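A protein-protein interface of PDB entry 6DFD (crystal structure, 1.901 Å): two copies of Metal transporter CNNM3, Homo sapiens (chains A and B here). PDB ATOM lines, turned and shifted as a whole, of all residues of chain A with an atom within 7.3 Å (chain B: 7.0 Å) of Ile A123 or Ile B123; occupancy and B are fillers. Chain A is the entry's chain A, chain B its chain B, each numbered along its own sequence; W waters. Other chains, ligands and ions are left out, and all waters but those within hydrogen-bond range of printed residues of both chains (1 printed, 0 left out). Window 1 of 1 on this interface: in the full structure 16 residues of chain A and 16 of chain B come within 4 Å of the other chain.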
ATOM      1  N   ARG A 104      -4.475  20.492 -16.459  1.00  0.00           N
ATOM      2  CA  ARG A 104      -3.182  21.125 -16.234  1.00  0.00           C
ATOM      3  C   ARG A 104      -2.628  21.693 -17.528  1.00  0.00           C
ATOM      4  O   ARG A 104      -2.648  21.035 -18.571  1.00  0.00           O
ATOM      5  CB  ARG A 104      -2.180  20.120 -15.664  1.00  0.00           C
ATOM      6  CG  ARG A 104      -2.285  19.846 -14.186  1.00  0.00           C
ATOM      7  CD  ARG A 104      -1.020  19.135 -13.718  1.00  0.00           C
ATOM      8  NE  ARG A 104      -0.110  20.051 -13.036  1.00  0.00           N
ATOM      9  CZ  ARG A 104      -0.056  20.223 -11.718  1.00  0.00           C
ATOM     10  NH1 ARG A 104      -0.855  19.534 -10.906  1.00  0.00           N
ATOM     11  NH2 ARG A 104       0.807  21.091 -11.208  1.00  0.00           N
ATOM     12  N   VAL A 121      -9.849  16.377  -8.049  1.00  0.00           N
ATOM     13  CA  VAL A 121      -8.926  17.456  -8.343  1.00  0.00           C
ATOM     14  C   VAL A 121      -7.525  16.927  -8.104  1.00  0.00           C
ATOM     15  O   VAL A 121      -7.257  16.335  -7.051  1.00  0.00           O
ATOM     16  CB  VAL A 121      -9.188  18.684  -7.453  1.00  0.00           C
ATOM     17  CG1 VAL A 121      -8.307  19.840  -7.876  1.00  0.00           C
ATOM     18  CG2 VAL A 121     -10.653  19.078  -7.487  1.00  0.00           C
ATOM     19  N   GLU A 122      -6.633  17.144  -9.064  1.00  0.00           N
ATOM     20  CA  GLU A 122      -5.209  16.918  -8.852  1.00  0.00           C
ATOM     21  C   GLU A 122      -4.504  18.247  -9.078  1.00  0.00           C
ATOM     22  O   GLU A 122      -4.658  18.859 -10.141  1.00  0.00           O
ATOM     23  CB  GLU A 122      -4.670  15.816  -9.769  1.00  0.00           C
ATOM     24  CG  GLU A 122      -4.627  16.160 -11.227  1.00  0.00           C
ATOM     25  CD  GLU A 122      -3.241  16.573 -11.674  1.00  0.00           C
ATOM     26  OE1 GLU A 122      -3.034  17.778 -11.919  1.00  0.00           O
ATOM     27  OE2 GLU A 122      -2.359  15.693 -11.762  1.00  0.00           O
ATOM     28  N   ILE A 123      -3.750  18.706  -8.078  1.00  0.00           N
ATOM     29  CA  ILE A 123      -3.399  20.119  -8.006  1.00  0.00           C
ATOM     30  C   ILE A 123      -2.006  20.301  -7.418  1.00  0.00           C
ATOM     31  O   ILE A 123      -1.545  19.515  -6.582  1.00  0.00           O
ATOM     32  CB  ILE A 123      -4.453  20.895  -7.183  1.00  0.00           C
ATOM     33  CG1 ILE A 123      -4.135  22.391  -7.195  1.00  0.00           C
ATOM     34  CG2 ILE A 123      -4.518  20.365  -5.765  1.00  0.00           C
ATOM     35  CD1 ILE A 123      -5.344  23.257  -6.976  1.00  0.00           C
ATOM     36  N   GLY A 124      -1.338  21.362  -7.875  1.00  0.00           N
ATOM     37  CA  GLY A 124      -0.059  21.762  -7.327  1.00  0.00           C
ATOM     38  C   GLY A 124       1.095  21.019  -7.969  1.00  0.00           C
ATOM     39  O   GLY A 124       0.929  20.158  -8.837  1.00  0.00           O
ATOM     40  N   LYS A 125       2.303  21.375  -7.524  1.00  0.00           N
ATOM     41  CA  LYS A 125       3.511  20.765  -8.074  1.00  0.00           C
ATOM     42  C   LYS A 125       3.592  19.280  -7.749  1.00  0.00           C
ATOM     43  O   LYS A 125       4.227  18.521  -8.489  1.00  0.00           O
ATOM     44  CB  LYS A 125       4.760  21.481  -7.548  1.00  0.00           C
ATOM     45  CG  LYS A 125       4.952  22.898  -8.079  1.00  0.00           C
ATOM     46  CD  LYS A 125       4.409  23.928  -7.104  1.00  0.00           C
ATOM     47  CE  LYS A 125       4.172  25.285  -7.748  1.00  0.00           C
ATOM     48  NZ  LYS A 125       3.100  26.039  -7.037  1.00  0.00           N
ATOM     49  N   GLU A 126       2.972  18.848  -6.652  1.00  0.00           N
ATOM     50  CA  GLU A 126       2.953  17.435  -6.299  1.00  0.00           C
ATOM     51  C   GLU A 126       1.772  16.696  -6.907  1.00  0.00           C
ATOM     52  O   GLU A 126       1.708  15.468  -6.799  1.00  0.00           O
ATOM     53  CB  GLU A 126       2.910  17.268  -4.777  1.00  0.00           C
ATOM     54  CG  GLU A 126       4.029  17.976  -4.035  1.00  0.00           C
ATOM     55  CD  GLU A 126       4.054  17.617  -2.563  1.00  0.00           C
ATOM     56  OE1 GLU A 126       3.882  16.421  -2.239  1.00  0.00           O
ATOM     57  OE2 GLU A 126       4.234  18.526  -1.728  1.00  0.00           O
ATOM     58  N   GLY A 127       0.837  17.409  -7.527  1.00  0.00           N
ATOM     59  CA  GLY A 127      -0.340  16.778  -8.079  1.00  0.00           C
ATOM     60  C   GLY A 127      -1.098  16.011  -7.017  1.00  0.00           C
ATOM     61  O   GLY A 127      -1.491  14.860  -7.231  1.00  0.00           O
ATOM     62  N   LEU A 128      -1.299  16.630  -5.856  1.00  0.00           N
ATOM     63  CA  LEU A 128      -2.086  15.973  -4.822  1.00  0.00           C
ATOM     64  C   LEU A 128      -3.513  15.799  -5.316  1.00  0.00           C
ATOM     65  O   LEU A 128      -4.051  16.657  -6.016  1.00  0.00           O
ATOM     66  CB  LEU A 128      -2.074  16.780  -3.521  1.00  0.00           C
ATOM     67  CG  LEU A 128      -0.706  17.021  -2.871  1.00  0.00           C
ATOM     68  CD1 LEU A 128      -0.879  17.757  -1.557  1.00  0.00           C
ATOM     69  CD2 LEU A 128       0.042  15.715  -2.651  1.00  0.00           C
ATOM     70  N   LYS A 129      -4.128  14.682  -4.944  1.00  0.00           N
ATOM     71  CA  LYS A 129      -5.448  14.313  -5.434  1.00  0.00           C
ATOM     72  C   LYS A 129      -6.426  14.311  -4.277  1.00  0.00           C
ATOM     73  O   LYS A 129      -6.149  13.722  -3.225  1.00  0.00           O
ATOM     74  CB  LYS A 129      -5.431  12.933  -6.096  1.00  0.00           C
ATOM     75  CG  LYS A 129      -5.200  12.952  -7.595  1.00  0.00           C
ATOM     76  CD  LYS A 129      -4.470  11.695  -8.072  1.00  0.00           C
ATOM     77  CE  LYS A 129      -5.145  10.404  -7.617  1.00  0.00           C
ATOM     78  NZ  LYS A 129      -4.250   9.229  -7.818  1.00  0.00           N
ATOM     79  N   PHE A 130      -7.565  14.968  -4.466  1.00  0.00           N
ATOM     80  CA  PHE A 130      -8.639  14.838  -3.498  1.00  0.00           C
ATOM     81  C   PHE A 130      -9.970  15.115  -4.181  1.00  0.00           C
ATOM     82  O   PHE A 130     -10.034  15.707  -5.261  1.00  0.00           O
ATOM     83  CB  PHE A 130      -8.431  15.752  -2.286  1.00  0.00           C
ATOM     84  CG  PHE A 130      -8.053  17.159  -2.634  1.00  0.00           C
ATOM     85  CD1 PHE A 130      -9.023  18.093  -2.945  1.00  0.00           C
ATOM     86  CD2 PHE A 130      -6.726  17.547  -2.636  1.00  0.00           C
ATOM     87  CE1 PHE A 130      -8.674  19.395  -3.263  1.00  0.00           C
ATOM     88  CE2 PHE A 130      -6.368  18.841  -2.949  1.00  0.00           C
ATOM     89  CZ  PHE A 130      -7.342  19.769  -3.264  1.00  0.00           C
ATOM     90  N   TYR A 138     -13.811  26.806  -9.085  1.00  0.00           N
ATOM     91  CA  TYR A 138     -12.553  26.698  -9.811  1.00  0.00           C
ATOM     92  C   TYR A 138     -12.496  27.809 -10.841  1.00  0.00           C
ATOM     93  O   TYR A 138     -13.523  28.341 -11.263  1.00  0.00           O
ATOM     94  CB  TYR A 138     -12.416  25.338 -10.524  1.00  0.00           C
ATOM     95  CG  TYR A 138     -12.761  24.204  -9.601  1.00  0.00           C
ATOM     96  CD1 TYR A 138     -11.789  23.609  -8.812  1.00  0.00           C
ATOM     97  CD2 TYR A 138     -14.075  23.790  -9.450  1.00  0.00           C
ATOM     98  CE1 TYR A 138     -12.113  22.607  -7.915  1.00  0.00           C
ATOM     99  CE2 TYR A 138     -14.410  22.796  -8.554  1.00  0.00           C
ATOM    100  CZ  TYR A 138     -13.421  22.209  -7.788  1.00  0.00           C
ATOM    101  OH  TYR A 138     -13.740  21.217  -6.878  1.00  0.00           O
ATOM    102  N   ASP A 180      -2.976  25.064 -12.831  1.00  0.00           N
ATOM    103  CA  ASP A 180      -2.086  24.029 -12.309  1.00  0.00           C
ATOM    104  C   ASP A 180      -2.882  22.927 -11.628  1.00  0.00           C
ATOM    105  O   ASP A 180      -2.481  22.387 -10.594  1.00  0.00           O
ATOM    106  CB  ASP A 180      -1.059  24.626 -11.351  1.00  0.00           C
ATOM    107  CG  ASP A 180      -1.686  25.161 -10.085  1.00  0.00           C
ATOM    108  OD1 ASP A 180      -2.929  25.268 -10.035  1.00  0.00           O
ATOM    109  OD2 ASP A 180      -0.934  25.465  -9.135  1.00  0.00           O
ATOM    110  N   TYR A 181      -4.041  22.599 -12.190  1.00  0.00           N
ATOM    111  CA  TYR A 181      -4.867  21.531 -11.658  1.00  0.00           C
ATOM    112  C   TYR A 181      -5.665  20.906 -12.786  1.00  0.00           C
ATOM    113  O   TYR A 181      -5.913  21.524 -13.825  1.00  0.00           O
ATOM    114  CB  TYR A 181      -5.816  22.021 -10.558  1.00  0.00           C
ATOM    115  CG  TYR A 181      -6.521  23.334 -10.843  1.00  0.00           C
ATOM    116  CD1 TYR A 181      -5.981  24.541 -10.414  1.00  0.00           C
ATOM    117  CD2 TYR A 181      -7.739  23.365 -11.512  1.00  0.00           C
ATOM    118  CE1 TYR A 181      -6.626  25.746 -10.659  1.00  0.00           C
ATOM    119  CE2 TYR A 181      -8.392  24.565 -11.761  1.00  0.00           C
ATOM    120  CZ  TYR A 181      -7.830  25.751 -11.331  1.00  0.00           C
ATOM    121  OH  TYR A 181      -8.475  26.947 -11.570  1.00  0.00           O
ATOM    122  N   THR A 182      -6.051  19.658 -12.565  1.00  0.00           N
ATOM    123  CA  THR A 182      -6.997  18.959 -13.412  1.00  0.00           C
ATOM    124  C   THR A 182      -8.210  18.634 -12.561  1.00  0.00           C
ATOM    125  O   THR A 182      -8.071  18.255 -11.391  1.00  0.00           O
ATOM    126  CB  THR A 182      -6.377  17.677 -14.000  1.00  0.00           C
ATOM    127  OG1 THR A 182      -5.145  18.004 -14.652  1.00  0.00           O
ATOM    128  CG2 THR A 182      -7.309  17.020 -15.001  1.00  0.00           C
ATOM    129  N   VAL A 183      -9.396  18.797 -13.145  1.00  0.00           N
ATOM    130  CA  VAL A 183     -10.653  18.554 -12.445  1.00  0.00           C
ATOM    131  C   VAL A 183     -11.503  17.648 -13.316  1.00  0.00           C
ATOM    132  O   VAL A 183     -11.821  18.000 -14.459  1.00  0.00           O
ATOM    133  CB  VAL A 183     -11.404  19.859 -12.128  1.00  0.00           C
ATOM    134  CG1 VAL A 183     -12.729  19.554 -11.442  1.00  0.00           C
ATOM    135  CG2 VAL A 183     -10.546  20.762 -11.259  1.00  0.00           C
ATOM    136  N   ARG B 104       4.026  27.011   3.348  1.00  0.00           N
ATOM    137  CA  ARG B 104       4.894  27.306   2.215  1.00  0.00           C
ATOM    138  C   ARG B 104       6.258  27.808   2.665  1.00  0.00           C
ATOM    139  O   ARG B 104       7.222  27.723   1.896  1.00  0.00           O
ATOM    140  CB  ARG B 104       4.248  28.347   1.298  1.00  0.00           C
ATOM    141  CG  ARG B 104       2.894  27.955   0.722  1.00  0.00           C
ATOM    142  CD  ARG B 104       2.416  29.009  -0.264  1.00  0.00           C
ATOM    143  NE  ARG B 104       1.088  28.733  -0.811  1.00  0.00           N
ATOM    144  CZ  ARG B 104       0.848  28.216  -2.016  1.00  0.00           C
ATOM    145  NH1 ARG B 104       1.842  27.904  -2.838  1.00  0.00           N
ATOM    146  NH2 ARG B 104      -0.401  28.014  -2.407  1.00  0.00           N
ATOM    147  N   VAL B 121      -6.901  23.752   3.459  1.00  0.00           N
ATOM    148  CA  VAL B 121      -5.763  23.641   2.559  1.00  0.00           C
ATOM    149  C   VAL B 121      -5.858  24.769   1.547  1.00  0.00           C
ATOM    150  O   VAL B 121      -6.863  24.882   0.838  1.00  0.00           O
ATOM    151  CB  VAL B 121      -5.738  22.284   1.835  1.00  0.00           C
ATOM    152  CG1 VAL B 121      -4.473  22.150   0.996  1.00  0.00           C
ATOM    153  CG2 VAL B 121      -5.872  21.131   2.827  1.00  0.00           C
ATOM    154  N   GLU B 122      -4.815  25.589   1.458  1.00  0.00           N
ATOM    155  CA  GLU B 122      -4.671  26.515   0.339  1.00  0.00           C
ATOM    156  C   GLU B 122      -3.497  26.023  -0.499  1.00  0.00           C
ATOM    157  O   GLU B 122      -2.381  25.898   0.015  1.00  0.00           O
ATOM    158  CB  GLU B 122      -4.469  27.956   0.816  1.00  0.00           C
ATOM    159  CG  GLU B 122      -3.098  28.255   1.396  1.00  0.00           C
ATOM    160  CD  GLU B 122      -2.080  28.663   0.345  1.00  0.00           C
ATOM    161  OE1 GLU B 122      -2.475  28.898  -0.818  1.00  0.00           O
ATOM    162  OE2 GLU B 122      -0.877  28.734   0.682  1.00  0.00           O
ATOM    163  N   ILE B 123      -3.755  25.713  -1.771  1.00  0.00           N
ATOM    164  CA  ILE B 123      -2.817  24.935  -2.575  1.00  0.00           C
ATOM    165  C   ILE B 123      -2.763  25.473  -3.998  1.00  0.00           C
ATOM    166  O   ILE B 123      -3.782  25.889  -4.560  1.00  0.00           O
ATOM    167  CB  ILE B 123      -3.201  23.440  -2.580  1.00  0.00           C
ATOM    168  CG1 ILE B 123      -2.175  22.621  -3.364  1.00  0.00           C
ATOM    169  CG2 ILE B 123      -4.590  23.247  -3.170  1.00  0.00           C
ATOM    170  CD1 ILE B 123      -2.227  21.138  -3.043  1.00  0.00           C
ATOM    171  N   GLY B 124      -1.568  25.441  -4.586  1.00  0.00           N
ATOM    172  CA  GLY B 124      -1.375  25.819  -5.967  1.00  0.00           C
ATOM    173  C   GLY B 124      -1.000  27.281  -6.127  1.00  0.00           C
ATOM    174  O   GLY B 124      -1.040  28.081  -5.190  1.00  0.00           O
ATOM    175  N   LYS B 125      -0.618  27.630  -7.358  1.00  0.00           N
ATOM    176  CA  LYS B 125      -0.314  29.024  -7.661  1.00  0.00           C
ATOM    177  C   LYS B 125      -1.554  29.895  -7.505  1.00  0.00           C
ATOM    178  O   LYS B 125      -1.466  31.041  -7.047  1.00  0.00           O
ATOM    179  CB  LYS B 125       0.266  29.143  -9.072  1.00  0.00           C
ATOM    180  CG  LYS B 125      -0.639  28.622 -10.179  1.00  0.00           C
ATOM    181  CD  LYS B 125       0.047  28.718 -11.534  1.00  0.00           C
ATOM    182  CE  LYS B 125      -0.886  28.321 -12.668  1.00  0.00           C
ATOM    183  NZ  LYS B 125      -0.287  28.586 -14.007  1.00  0.00           N
ATOM    184  N   GLU B 126      -2.722  29.369  -7.876  1.00  0.00           N
ATOM    185  CA  GLU B 126      -3.980  30.040  -7.575  1.00  0.00           C
ATOM    186  C   GLU B 126      -4.344  29.955  -6.100  1.00  0.00           C
ATOM    187  O   GLU B 126      -5.282  30.637  -5.671  1.00  0.00           O
ATOM    188  CB  GLU B 126      -5.121  29.437  -8.398  1.00  0.00           C
ATOM    189  CG  GLU B 126      -5.714  30.366  -9.441  1.00  0.00           C
ATOM    190  CD  GLU B 126      -6.956  29.780 -10.103  1.00  0.00           C
ATOM    191  OE1 GLU B 126      -6.823  28.768 -10.823  1.00  0.00           O
ATOM    192  OE2 GLU B 126      -8.063  30.328  -9.893  1.00  0.00           O
ATOM    193  N   GLY B 127      -3.646  29.131  -5.328  1.00  0.00           N
ATOM    194  CA  GLY B 127      -3.957  29.005  -3.910  1.00  0.00           C
ATOM    195  C   GLY B 127      -5.403  28.665  -3.642  1.00  0.00           C
ATOM    196  O   GLY B 127      -6.009  29.209  -2.709  1.00  0.00           O
ATOM    197  N   LEU B 128      -5.984  27.780  -4.450  1.00  0.00           N
ATOM    198  CA  LEU B 128      -7.353  27.352  -4.204  1.00  0.00           C
ATOM    199  C   LEU B 128      -7.480  26.829  -2.781  1.00  0.00           C
ATOM    200  O   LEU B 128      -6.615  26.098  -2.289  1.00  0.00           O
ATOM    201  CB  LEU B 128      -7.774  26.275  -5.208  1.00  0.00           C
ATOM    202  CG  LEU B 128      -8.600  26.757  -6.407  1.00  0.00           C
ATOM    203  CD1 LEU B 128      -7.883  27.867  -7.135  1.00  0.00           C
ATOM    204  CD2 LEU B 128      -8.900  25.630  -7.381  1.00  0.00           C
ATOM    205  N   LYS B 129      -8.555  27.235  -2.114  1.00  0.00           N
ATOM    206  CA  LYS B 129      -8.831  26.827  -0.746  1.00  0.00           C
ATOM    207  C   LYS B 129      -9.852  25.700  -0.740  1.00  0.00           C
ATOM    208  O   LYS B 129     -10.826  25.723  -1.498  1.00  0.00           O
ATOM    209  CB  LYS B 129      -9.356  27.995   0.091  1.00  0.00           C
ATOM    210  CG  LYS B 129      -8.302  29.006   0.502  1.00  0.00           C
ATOM    211  CD  LYS B 129      -8.878  29.990   1.510  1.00  0.00           C
ATOM    212  CE  LYS B 129      -8.034  31.247   1.631  1.00  0.00           C
ATOM    213  NZ  LYS B 129      -8.725  32.297   2.432  1.00  0.00           N
ATOM    214  N   PHE B 130      -9.627  24.719   0.128  1.00  0.00           N
ATOM    215  CA  PHE B 130     -10.533  23.598   0.286  1.00  0.00           C
ATOM    216  C   PHE B 130     -10.569  23.191   1.749  1.00  0.00           C
ATOM    217  O   PHE B 130      -9.601  23.383   2.488  1.00  0.00           O
ATOM    218  CB  PHE B 130     -10.106  22.403  -0.568  1.00  0.00           C
ATOM    219  CG  PHE B 130      -9.927  22.736  -2.021  1.00  0.00           C
ATOM    220  CD1 PHE B 130     -11.017  23.083  -2.805  1.00  0.00           C
ATOM    221  CD2 PHE B 130      -8.671  22.701  -2.604  1.00  0.00           C
ATOM    222  CE1 PHE B 130     -10.856  23.390  -4.140  1.00  0.00           C
ATOM    223  CE2 PHE B 130      -8.505  23.003  -3.939  1.00  0.00           C
ATOM    224  CZ  PHE B 130      -9.599  23.345  -4.708  1.00  0.00           C
ATOM    225  N   ASN B 132     -10.606  19.859   3.602  1.00  0.00           N
ATOM    226  CA  ASN B 132     -10.304  18.466   3.330  1.00  0.00           C
ATOM    227  C   ASN B 132     -10.432  17.652   4.609  1.00  0.00           C
ATOM    228  O   ASN B 132     -10.242  18.168   5.713  1.00  0.00           O
ATOM    229  CB  ASN B 132      -8.896  18.340   2.744  1.00  0.00           C
ATOM    230  CG  ASN B 132      -8.845  18.736   1.276  1.00  0.00           C
ATOM    231  OD1 ASN B 132      -9.841  19.199   0.715  1.00  0.00           O
ATOM    232  ND2 ASN B 132      -7.685  18.560   0.650  1.00  0.00           N
ATOM    233  N   TYR B 138      -0.843  14.442   1.965  1.00  0.00           N
ATOM    234  CA  TYR B 138       0.027  15.577   1.721  1.00  0.00           C
ATOM    235  C   TYR B 138       1.467  15.103   1.842  1.00  0.00           C
ATOM    236  O   TYR B 138       1.756  14.095   2.492  1.00  0.00           O
ATOM    237  CB  TYR B 138      -0.275  16.709   2.715  1.00  0.00           C
ATOM    238  CG  TYR B 138      -1.754  16.983   2.807  1.00  0.00           C
ATOM    239  CD1 TYR B 138      -2.570  16.220   3.633  1.00  0.00           C
ATOM    240  CD2 TYR B 138      -2.345  17.960   2.026  1.00  0.00           C
ATOM    241  CE1 TYR B 138      -3.935  16.442   3.687  1.00  0.00           C
ATOM    242  CE2 TYR B 138      -3.705  18.190   2.081  1.00  0.00           C
ATOM    243  CZ  TYR B 138      -4.490  17.430   2.910  1.00  0.00           C
ATOM    244  OH  TYR B 138      -5.848  17.668   2.951  1.00  0.00           O
ATOM    245  N   ASP B 180       3.937  23.763  -2.024  1.00  0.00           N
ATOM    246  CA  ASP B 180       3.083  24.799  -2.601  1.00  0.00           C
ATOM    247  C   ASP B 180       1.702  24.798  -1.975  1.00  0.00           C
ATOM    248  O   ASP B 180       0.685  24.882  -2.675  1.00  0.00           O
ATOM    249  CB  ASP B 180       2.990  24.608  -4.110  1.00  0.00           C
ATOM    250  CG  ASP B 180       2.320  23.301  -4.491  1.00  0.00           C
ATOM    251  OD1 ASP B 180       2.415  22.330  -3.711  1.00  0.00           O
ATOM    252  OD2 ASP B 180       1.698  23.248  -5.571  1.00  0.00           O
ATOM    253  N   TYR B 181       1.631  24.681  -0.655  1.00  0.00           N
ATOM    254  CA  TYR B 181       0.347  24.694   0.028  1.00  0.00           C
ATOM    255  C   TYR B 181       0.565  24.955   1.508  1.00  0.00           C
ATOM    256  O   TYR B 181       1.676  24.826   2.028  1.00  0.00           O
ATOM    257  CB  TYR B 181      -0.414  23.377  -0.170  1.00  0.00           C
ATOM    258  CG  TYR B 181       0.434  22.122  -0.052  1.00  0.00           C
ATOM    259  CD1 TYR B 181       0.972  21.516  -1.182  1.00  0.00           C
ATOM    260  CD2 TYR B 181       0.679  21.534   1.183  1.00  0.00           C
ATOM    261  CE1 TYR B 181       1.741  20.362  -1.084  1.00  0.00           C
ATOM    262  CE2 TYR B 181       1.448  20.382   1.291  1.00  0.00           C
ATOM    263  CZ  TYR B 181       1.975  19.799   0.154  1.00  0.00           C
ATOM    264  OH  TYR B 181       2.738  18.652   0.256  1.00  0.00           O
ATOM    265  N   THR B 182      -0.519  25.335   2.176  1.00  0.00           N
ATOM    266  CA  THR B 182      -0.558  25.381   3.628  1.00  0.00           C
ATOM    267  C   THR B 182      -1.766  24.583   4.092  1.00  0.00           C
ATOM    268  O   THR B 182      -2.833  24.630   3.468  1.00  0.00           O
ATOM    269  CB  THR B 182      -0.628  26.820   4.168  1.00  0.00           C
ATOM    270  OG1 THR B 182      -1.936  27.357   3.951  1.00  0.00           O
ATOM    271  CG2 THR B 182       0.400  27.697   3.479  1.00  0.00           C
HETATM  272  O   HOH W   1       1.132  20.091  -4.864  1.00  0.00           O
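Among the printed residues, merely in contact across the chains: Gly A124 with Asp B180 (2.9 Å), Asp A180 with Gly B124 (3.2 Å), Phe A130 with Phe B130 (3.3 Å), Phe A130 with Asn B132 (3.6 Å), Ile A123 with Ile B123 (3.6 Å), Leu A128 with Tyr B181 (3.7 Å), Tyr A138 with Leu B128 (3.8 Å), Leu A128 with Tyr B138 (3.9 Å), Leu A128 with Ile B123 (3.9 Å) and Tyr A181 with Leu B128 (3.99 Å).
OD2 of Asp B180 lies within salt-bridge range of NZ of Lys A125 (3.5 Å). OE2 of Glu A126 is in hydrogen-bond range of OH of Tyr B181 (2.5 Å). The side-chain carboxylate (OD2) of Asp A180 lies within hydrogen-bond range of the backbone NH (N) of Lys B125 (2.8 Å). OH of Tyr A181 is in hydrogen-bond range of OE1 of Glu B126, 2.6 Å away.
Of the 16 printed residues of chain A, 9 touch a printed residue of chain B. Printed residues of chain A that touch a printed residue of chain B: Ile A123, Gly A124, Lys A125, Glu A126, Leu A128, Phe A130, Tyr A138, Asp A180 and Tyr A181. Hydrophobic or aromatic side chains of chain B within 4 Å of the printed part of chain A: Ile B123, Leu B128, Phe B130, Tyr B138 and Tyr B181. Among the printed residues, Asp or Glu carboxylates within 4 Å of a Lys or Arg side-chain nitrogen of the other chain: Lys A125 with Asp B180 (3.5 Å).
Water W1 lies within hydrogen-bond range of the side-chain carboxylate of Asp B180 (2.8 Å), the backbone NH of Glu A126 (2.9 Å), the backbone NH of Lys A125 (3.2 Å) and the backbone carbonyl oxygen of Ile A123 (3.2 Å).
Ile B123 touches its own counterpart, Ile A123. Lys A125 touches Asp B180, and with the chains exchanged Asp A180 touches Lys B125. Glu A126 touches Tyr B181, and with the chains exchanged Tyr A181 touches Glu B126. Leu A128 touches Tyr B181, and with the chains exchanged Tyr A181 touches Leu B128. Positions printed for both chains: 104, 121, 122, 123, 124, 125, 126, 127, 128, 129, 130, 138, 180, 181 and 182.
O of Gly A124 sits at hydrogen-bond distance from NH2 of Arg A104, 2.6 Å away. O of Gly B124 sits at hydrogen-bond distance from NH2 of Arg B104 (2.9 Å). O of Asp B180 sits close to NH1 of Arg B104 (3.2 Å). N of Phe B130 is in hydrogen-bond range of O of Val B121 (2.9 Å). O of Ile B123 is in hydrogen-bond range of N of Leu B128 (2.9 Å). The side-chain amide nitrogen (ND2) of Asn B132 lies within hydrogen-bond range of the side-chain hydroxyl (OH) of Tyr B138, 3.1 Å away.
Printed residues of chain B within 4 Å of Glu A126: Tyr B181 (2.5 Å). Thr A182 touches none of the printed residues of chain B. Printed residues of chain A within 4 Å of Ile B123: Ile A123 (3.6 Å) and Leu A128 (3.9 Å). Printed residues of chain A within 4 Å of Glu B126: Tyr A181. The nearest residue of chain A that does not touch Ile B123 is Phe A130 (4.4 Å). The nearest printed residue of chain A that does not touch Leu B128 is Ile A123 (4.3 Å).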
